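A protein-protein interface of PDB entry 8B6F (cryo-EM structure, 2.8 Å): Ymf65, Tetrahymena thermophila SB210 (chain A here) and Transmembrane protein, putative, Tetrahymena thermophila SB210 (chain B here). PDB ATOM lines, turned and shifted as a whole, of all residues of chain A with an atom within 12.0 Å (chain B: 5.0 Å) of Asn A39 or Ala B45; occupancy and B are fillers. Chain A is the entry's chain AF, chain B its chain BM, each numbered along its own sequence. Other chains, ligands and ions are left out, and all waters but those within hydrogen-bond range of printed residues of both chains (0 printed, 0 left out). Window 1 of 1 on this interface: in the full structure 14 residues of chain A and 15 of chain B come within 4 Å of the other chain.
NE1 of Trp A41 is in hydrogen-bond range of OG of Ser B32 (3.0 Å).
The side-chain hydroxyl (OG) of Ser B32 is in hydrogen-bond range of the side-chain carboxylate (OD1) of Asp A42, 2.7 Å away.
N of Asn A39 sits at hydrogen-bond distance from OD2 of Asp A42, 2.7 Å away.
Gln B48 touches Lys A37 (OE1 to NZ, 3.98 Å).
Ala B45 touches Asn A39.
CB of Gln B48 touches ND2 of Asn A39 (3.6 Å).
Trp A41 touches Lys B44.
Trp A41 touches Gln B48.
Asn A39 touches just these residues of chain B: Ala B45 (3.9 Å) and Gln B48 (3.6 Å).
Of the printed residues of chain B, Trp A41 touches Ser B32, Lys B44 and Gln B48.
Of the printed residues of chain B, Asp A42 touches Ser B32.
Ser B32 touches just these residues of chain A: Trp A41 and Asp A42.
No residue of chain A comes within 4 Å of Val B41.
Of chain A, only Asn A39 (3.9 Å) comes within 4 Å of Ala B45.
Trp B46 touches none of the printed residues of chain A.
The nearest printed residue of chain B that does not touch Asp A42 is Ile B33 (5.1 Å).
Printed residues of chain B that touch a printed residue of chain A: Ser B32, Lys B44, Ala B45 and Gln B48.
Printed residues of chain A that touch a printed residue of chain B: Lys A37, Asn A39, Trp A41 and Asp A42.
Among the printed residues, no Asp or Glu carboxylate lies within 4 Å of a Lys or Arg side-chain nitrogen of the other chain.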
ATOM      1  N   VAL A  35      10.784  11.467  17.387  1.00  0.00           N
ATOM      2  CA  VAL A  35      11.443  11.976  16.188  1.00  0.00           C
ATOM      3  C   VAL A  35      12.119  10.807  15.480  1.00  0.00           C
ATOM      4  O   VAL A  35      13.102  10.251  15.976  1.00  0.00           O
ATOM      5  CB  VAL A  35      12.453  13.079  16.528  1.00  0.00           C
ATOM      6  CG1 VAL A  35      13.134  13.591  15.267  1.00  0.00           C
ATOM      7  CG2 VAL A  35      11.764  14.215  17.259  1.00  0.00           C
ATOM      8  N   ASN A  36      11.595  10.438  14.310  1.00  0.00           N
ATOM      9  CA  ASN A  36      12.173   9.361  13.506  1.00  0.00           C
ATOM     10  C   ASN A  36      11.927   9.705  12.041  1.00  0.00           C
ATOM     11  O   ASN A  36      10.845   9.436  11.512  1.00  0.00           O
ATOM     12  CB  ASN A  36      11.570   8.016  13.881  1.00  0.00           C
ATOM     13  CG  ASN A  36      12.212   6.859  13.142  1.00  0.00           C
ATOM     14  OD1 ASN A  36      13.239   7.019  12.487  1.00  0.00           O
ATOM     15  ND2 ASN A  36      11.609   5.683  13.251  1.00  0.00           N
ATOM     16  N   LYS A  37      12.931  10.294  11.395  1.00  0.00           N
ATOM     17  CA  LYS A  37      12.780  10.740  10.018  1.00  0.00           C
ATOM     18  C   LYS A  37      12.608   9.558   9.073  1.00  0.00           C
ATOM     19  O   LYS A  37      13.218   8.500   9.254  1.00  0.00           O
ATOM     20  CB  LYS A  37      13.994  11.567   9.597  1.00  0.00           C
ATOM     21  CG  LYS A  37      13.935  12.067   8.163  1.00  0.00           C
ATOM     22  CD  LYS A  37      15.172  12.873   7.808  1.00  0.00           C
ATOM     23  CE  LYS A  37      15.128  13.328   6.358  1.00  0.00           C
ATOM     24  NZ  LYS A  37      16.350  14.089   5.974  1.00  0.00           N
ATOM     25  N   LYS A  38      11.769   9.747   8.057  1.00  0.00           N
ATOM     26  CA  LYS A  38      11.552   8.764   7.002  1.00  0.00           C
ATOM     27  C   LYS A  38      12.166   9.310   5.718  1.00  0.00           C
ATOM     28  O   LYS A  38      11.624  10.237   5.110  1.00  0.00           O
ATOM     29  CB  LYS A  38      10.063   8.476   6.820  1.00  0.00           C
ATOM     30  CG  LYS A  38       9.747   7.526   5.673  1.00  0.00           C
ATOM     31  CD  LYS A  38       8.250   7.300   5.540  1.00  0.00           C
ATOM     32  CE  LYS A  38       7.929   6.450   4.322  1.00  0.00           C
ATOM     33  NZ  LYS A  38       6.467   6.220   4.170  1.00  0.00           N
ATOM     34  N   ASN A  39      13.290   8.732   5.309  1.00  0.00           N
ATOM     35  CA  ASN A  39      13.952   9.164   4.088  1.00  0.00           C
ATOM     36  C   ASN A  39      13.082   8.863   2.875  1.00  0.00           C
ATOM     37  O   ASN A  39      12.256   7.945   2.886  1.00  0.00           O
ATOM     38  CB  ASN A  39      15.310   8.481   3.949  1.00  0.00           C
ATOM     39  CG  ASN A  39      16.220   8.763   5.124  1.00  0.00           C
ATOM     40  OD1 ASN A  39      16.641   7.851   5.833  1.00  0.00           O
ATOM     41  ND2 ASN A  39      16.527  10.036   5.340  1.00  0.00           N
ATOM     42  N   ASN A  40      13.271   9.652   1.815  1.00  0.00           N
ATOM     43  CA  ASN A  40      12.418   9.516   0.637  1.00  0.00           C
ATOM     44  C   ASN A  40      12.491   8.115   0.048  1.00  0.00           C
ATOM     45  O   ASN A  40      11.537   7.666  -0.594  1.00  0.00           O
ATOM     46  CB  ASN A  40      12.802  10.553  -0.417  1.00  0.00           C
ATOM     47  CG  ASN A  40      12.469  11.965   0.013  1.00  0.00           C
ATOM     48  OD1 ASN A  40      12.464  12.280   1.201  1.00  0.00           O
ATOM     49  ND2 ASN A  40      12.178  12.826  -0.955  1.00  0.00           N
ATOM     50  N   TRP A  41      13.603   7.414   0.246  1.00  0.00           N
ATOM     51  CA  TRP A  41      13.736   6.045  -0.227  1.00  0.00           C
ATOM     52  C   TRP A  41      13.216   5.013   0.767  1.00  0.00           C
ATOM     53  O   TRP A  41      13.140   3.830   0.421  1.00  0.00           O
ATOM     54  CB  TRP A  41      15.202   5.753  -0.566  1.00  0.00           C
ATOM     55  CG  TRP A  41      16.139   5.944   0.584  1.00  0.00           C
ATOM     56  CD1 TRP A  41      16.472   5.026   1.533  1.00  0.00           C
ATOM     57  CD2 TRP A  41      16.867   7.138   0.905  1.00  0.00           C
ATOM     58  NE1 TRP A  41      17.363   5.575   2.423  1.00  0.00           N
ATOM     59  CE2 TRP A  41      17.621   6.868   2.059  1.00  0.00           C
ATOM     60  CE3 TRP A  41      16.953   8.406   0.325  1.00  0.00           C
ATOM     61  CZ2 TRP A  41      18.449   7.815   2.652  1.00  0.00           C
ATOM     62  CZ3 TRP A  41      17.778   9.349   0.914  1.00  0.00           C
ATOM     63  CH2 TRP A  41      18.516   9.047   2.067  1.00  0.00           C
ATOM     64  N   ASP A  42      12.866   5.421   1.985  1.00  0.00           N
ATOM     65  CA  ASP A  42      12.344   4.485   2.971  1.00  0.00           C
ATOM     66  C   ASP A  42      10.906   4.097   2.646  1.00  0.00           C
ATOM     67  O   ASP A  42      10.116   4.904   2.149  1.00  0.00           O
ATOM     68  CB  ASP A  42      12.408   5.087   4.374  1.00  0.00           C
ATOM     69  CG  ASP A  42      13.821   5.180   4.903  1.00  0.00           C
ATOM     70  OD1 ASP A  42      14.634   4.290   4.583  1.00  0.00           O
ATOM     71  OD2 ASP A  42      14.119   6.142   5.640  1.00  0.00           O
ATOM     72  N   LYS A  43      10.568   2.844   2.942  1.00  0.00           N
ATOM     73  CA  LYS A  43       9.236   2.303   2.714  1.00  0.00           C
ATOM     74  C   LYS A  43       8.635   1.891   4.050  1.00  0.00           C
ATOM     75  O   LYS A  43       9.298   1.223   4.850  1.00  0.00           O
ATOM     76  CB  LYS A  43       9.289   1.108   1.758  1.00  0.00           C
ATOM     77  CG  LYS A  43       7.931   0.516   1.416  1.00  0.00           C
ATOM     78  CD  LYS A  43       8.069  -0.635   0.428  1.00  0.00           C
ATOM     79  CE  LYS A  43       6.718  -1.246   0.100  1.00  0.00           C
ATOM     80  NZ  LYS A  43       6.832  -2.357  -0.883  1.00  0.00           N
ATOM     81  N   SER A  44       7.389   2.288   4.289  1.00  0.00           N
ATOM     82  CA  SER A  44       6.701   2.019   5.547  1.00  0.00           C
ATOM     83  C   SER A  44       5.792   0.810   5.376  1.00  0.00           C
ATOM     84  O   SER A  44       4.912   0.807   4.510  1.00  0.00           O
ATOM     85  CB  SER A  44       5.891   3.231   6.003  1.00  0.00           C
ATOM     86  OG  SER A  44       6.735   4.327   6.301  1.00  0.00           O
ATOM     87  N   ILE A  45       6.003  -0.212   6.207  1.00  0.00           N
ATOM     88  CA  ILE A  45       5.150  -1.393   6.160  1.00  0.00           C
ATOM     89  C   ILE A  45       3.735  -1.044   6.603  1.00  0.00           C
ATOM     90  O   ILE A  45       2.754  -1.593   6.087  1.00  0.00           O
ATOM     91  CB  ILE A  45       5.757  -2.522   7.014  1.00  0.00           C
ATOM     92  CG1 ILE A  45       4.970  -3.818   6.810  1.00  0.00           C
ATOM     93  CG2 ILE A  45       5.787  -2.125   8.488  1.00  0.00           C
ATOM     94  CD1 ILE A  45       5.584  -5.027   7.487  1.00  0.00           C
ATOM     95  N   SER A  46       3.606  -0.134   7.564  1.00  0.00           N
ATOM     96  CA  SER A  46       2.313   0.304   8.065  1.00  0.00           C
ATOM     97  C   SER A  46       2.334   1.816   8.228  1.00  0.00           C
ATOM     98  O   SER A  46       3.396   2.440   8.289  1.00  0.00           O
ATOM     99  CB  SER A  46       1.962  -0.379   9.394  1.00  0.00           C
ATOM    100  OG  SER A  46       2.984  -0.185  10.356  1.00  0.00           O
ATOM    101  N   LYS A  48       2.277   5.189  10.057  1.00  0.00           N
ATOM    102  CA  LYS A  48       2.741   5.576  11.381  1.00  0.00           C
ATOM    103  C   LYS A  48       1.589   6.100  12.227  1.00  0.00           C
ATOM    104  O   LYS A  48       0.727   6.840  11.747  1.00  0.00           O
ATOM    105  CB  LYS A  48       3.831   6.644  11.267  1.00  0.00           C
ATOM    106  CG  LYS A  48       4.311   7.185  12.606  1.00  0.00           C
ATOM    107  CD  LYS A  48       5.434   8.192  12.427  1.00  0.00           C
ATOM    108  CE  LYS A  48       5.907   8.731  13.765  1.00  0.00           C
ATOM    109  NZ  LYS A  48       7.000   9.728  13.602  1.00  0.00           N
ATOM    110  N   SER B  32      15.826   2.313   6.637  1.00  0.00           N
ATOM    111  CA  SER B  32      17.268   2.268   6.437  1.00  0.00           C
ATOM    112  C   SER B  32      18.018   2.354   7.759  1.00  0.00           C
ATOM    113  O   SER B  32      19.033   1.674   7.952  1.00  0.00           O
ATOM    114  CB  SER B  32      17.683   3.380   5.482  1.00  0.00           C
ATOM    115  OG  SER B  32      17.090   3.130   4.222  1.00  0.00           O
ATOM    116  N   ILE B  33      17.537   3.186   8.683  1.00  0.00           N
ATOM    117  CA  ILE B  33      18.242   3.381   9.946  1.00  0.00           C
ATOM    118  C   ILE B  33      18.256   2.094  10.756  1.00  0.00           C
ATOM    119  O   ILE B  33      19.230   1.805  11.460  1.00  0.00           O
ATOM    120  CB  ILE B  33      17.608   4.545  10.734  1.00  0.00           C
ATOM    121  CG1 ILE B  33      18.453   4.898  11.960  1.00  0.00           C
ATOM    122  CG2 ILE B  33      16.183   4.205  11.150  1.00  0.00           C
ATOM    123  CD1 ILE B  33      19.841   5.408  11.636  1.00  0.00           C
ATOM    124  N   VAL B  41      23.438   0.990   3.965  1.00  0.00           N
ATOM    125  CA  VAL B  41      22.107   1.569   4.134  1.00  0.00           C
ATOM    126  C   VAL B  41      22.021   2.307   5.463  1.00  0.00           C
ATOM    127  O   VAL B  41      21.498   3.425   5.542  1.00  0.00           O
ATOM    128  CB  VAL B  41      21.028   0.478   4.017  1.00  0.00           C
ATOM    129  CG1 VAL B  41      19.645   1.077   4.189  1.00  0.00           C
ATOM    130  CG2 VAL B  41      21.128  -0.229   2.678  1.00  0.00           C
ATOM    131  N   TRP B  42      22.523   1.688   6.532  1.00  0.00           N
ATOM    132  CA  TRP B  42      22.527   2.352   7.831  1.00  0.00           C
ATOM    133  C   TRP B  42      23.349   3.632   7.796  1.00  0.00           C
ATOM    134  O   TRP B  42      22.950   4.649   8.375  1.00  0.00           O
ATOM    135  CB  TRP B  42      23.067   1.416   8.911  1.00  0.00           C
ATOM    136  CG  TRP B  42      23.206   2.096  10.240  1.00  0.00           C
ATOM    137  CD1 TRP B  42      22.294   2.109  11.249  1.00  0.00           C
ATOM    138  CD2 TRP B  42      24.321   2.872  10.697  1.00  0.00           C
ATOM    139  NE1 TRP B  42      22.770   2.840  12.308  1.00  0.00           N
ATOM    140  CE2 TRP B  42      24.013   3.319  11.994  1.00  0.00           C
ATOM    141  CE3 TRP B  42      25.552   3.229  10.134  1.00  0.00           C
ATOM    142  CZ2 TRP B  42      24.889   4.105  12.740  1.00  0.00           C
ATOM    143  CZ3 TRP B  42      26.420   4.010  10.875  1.00  0.00           C
ATOM    144  CH2 TRP B  42      26.085   4.438  12.165  1.00  0.00           C
ATOM    145  N   PHE B  43      24.498   3.606   7.120  1.00  0.00           N
ATOM    146  CA  PHE B  43      25.331   4.801   7.057  1.00  0.00           C
ATOM    147  C   PHE B  43      24.619   5.925   6.322  1.00  0.00           C
ATOM    148  O   PHE B  43      24.703   7.090   6.727  1.00  0.00           O
ATOM    149  CB  PHE B  43      26.666   4.487   6.383  1.00  0.00           C
ATOM    150  CG  PHE B  43      27.552   5.686   6.232  1.00  0.00           C
ATOM    151  CD1 PHE B  43      28.220   6.204   7.327  1.00  0.00           C
ATOM    152  CD2 PHE B  43      27.709   6.302   5.003  1.00  0.00           C
ATOM    153  CE1 PHE B  43      29.035   7.312   7.202  1.00  0.00           C
ATOM    154  CE2 PHE B  43      28.522   7.412   4.870  1.00  0.00           C
ATOM    155  CZ  PHE B  43      29.186   7.918   5.971  1.00  0.00           C
ATOM    156  N   LYS B  44      23.920   5.603   5.234  1.00  0.00           N
ATOM    157  CA  LYS B  44      23.170   6.630   4.523  1.00  0.00           C
ATOM    158  C   LYS B  44      22.110   7.245   5.427  1.00  0.00           C
ATOM    159  O   LYS B  44      21.974   8.471   5.501  1.00  0.00           O
ATOM    160  CB  LYS B  44      22.532   6.029   3.272  1.00  0.00           C
ATOM    161  CG  LYS B  44      21.985   7.055   2.301  1.00  0.00           C
ATOM    162  CD  LYS B  44      21.322   6.376   1.115  1.00  0.00           C
ATOM    163  CE  LYS B  44      21.000   7.372   0.015  1.00  0.00           C
ATOM    164  NZ  LYS B  44      20.258   6.732  -1.107  1.00  0.00           N
ATOM    165  N   ALA B  45      21.333   6.404   6.112  1.00  0.00           N
ATOM    166  CA  ALA B  45      20.287   6.918   6.990  1.00  0.00           C
ATOM    167  C   ALA B  45      20.875   7.753   8.120  1.00  0.00           C
ATOM    168  O   ALA B  45      20.364   8.832   8.437  1.00  0.00           O
ATOM    169  CB  ALA B  45      19.462   5.763   7.554  1.00  0.00           C
ATOM    170  N   TRP B  46      21.953   7.266   8.740  1.00  0.00           N
ATOM    171  CA  TRP B  46      22.563   7.983   9.855  1.00  0.00           C
ATOM    172  C   TRP B  46      23.177   9.297   9.397  1.00  0.00           C
ATOM    173  O   TRP B  46      23.118  10.301  10.117  1.00  0.00           O
ATOM    174  CB  TRP B  46      23.620   7.113  10.532  1.00  0.00           C
ATOM    175  CG  TRP B  46      24.354   7.824  11.634  1.00  0.00           C
ATOM    176  CD1 TRP B  46      24.015   7.858  12.953  1.00  0.00           C
ATOM    177  CD2 TRP B  46      25.548   8.607  11.506  1.00  0.00           C
ATOM    178  NE1 TRP B  46      24.923   8.610  13.656  1.00  0.00           N
ATOM    179  CE2 TRP B  46      25.874   9.081  12.791  1.00  0.00           C
ATOM    180  CE3 TRP B  46      26.373   8.949  10.431  1.00  0.00           C
ATOM    181  CZ2 TRP B  46      26.989   9.880  13.030  1.00  0.00           C
ATOM    182  CZ3 TRP B  46      27.480   9.744  10.670  1.00  0.00           C
ATOM    183  CH2 TRP B  46      27.778  10.201  11.960  1.00  0.00           C
ATOM    184  N   LYS B  47      23.770   9.314   8.203  1.00  0.00           N
ATOM    185  CA  LYS B  47      24.315  10.560   7.677  1.00  0.00           C
ATOM    186  C   LYS B  47      23.215  11.587   7.463  1.00  0.00           C
ATOM    187  O   LYS B  47      23.383  12.763   7.801  1.00  0.00           O
ATOM    188  CB  LYS B  47      25.069  10.287   6.376  1.00  0.00           C
ATOM    189  CG  LYS B  47      25.470  11.536   5.608  1.00  0.00           C
ATOM    190  CD  LYS B  47      26.411  11.193   4.462  1.00  0.00           C
ATOM    191  CE  LYS B  47      26.629  12.384   3.540  1.00  0.00           C
ATOM    192  NZ  LYS B  47      25.417  12.706   2.734  1.00  0.00           N
ATOM    193  N   GLN B  48      22.080  11.168   6.905  1.00  0.00           N
ATOM    194  CA  GLN B  48      20.970  12.098   6.737  1.00  0.00           C
ATOM    195  C   GLN B  48      20.472  12.604   8.083  1.00  0.00           C
ATOM    196  O   GLN B  48      20.197  13.798   8.244  1.00  0.00           O
ATOM    197  CB  GLN B  48      19.838  11.430   5.961  1.00  0.00           C
ATOM    198  CG  GLN B  48      20.122  11.283   4.482  1.00  0.00           C
ATOM    199  CD  GLN B  48      20.427  12.610   3.820  1.00  0.00           C
ATOM    200  OE1 GLN B  48      19.555  13.467   3.691  1.00  0.00           O
ATOM    201  NE2 GLN B  48      21.675  12.790   3.408  1.00  0.00           N
ATOM    202  N   LYS B  49      20.339  11.706   9.061  1.00  0.00           N
ATOM    203  CA  LYS B  49      19.883  12.118  10.383  1.00  0.00           C
ATOM    204  C   LYS B  49      20.852  13.113  11.009  1.00  0.00           C
ATOM    205  O   LYS B  49      20.432  14.118  11.596  1.00  0.00           O
ATOM    206  CB  LYS B  49      19.716  10.896  11.285  1.00  0.00           C
ATOM    207  CG  LYS B  49      19.190  11.221  12.678  1.00  0.00           C
ATOM    208  CD  LYS B  49      19.098   9.981  13.553  1.00  0.00           C
ATOM    209  CE  LYS B  49      20.476   9.460  13.930  1.00  0.00           C
ATOM    210  NZ  LYS B  49      20.390   8.294  14.853  1.00  0.00           N
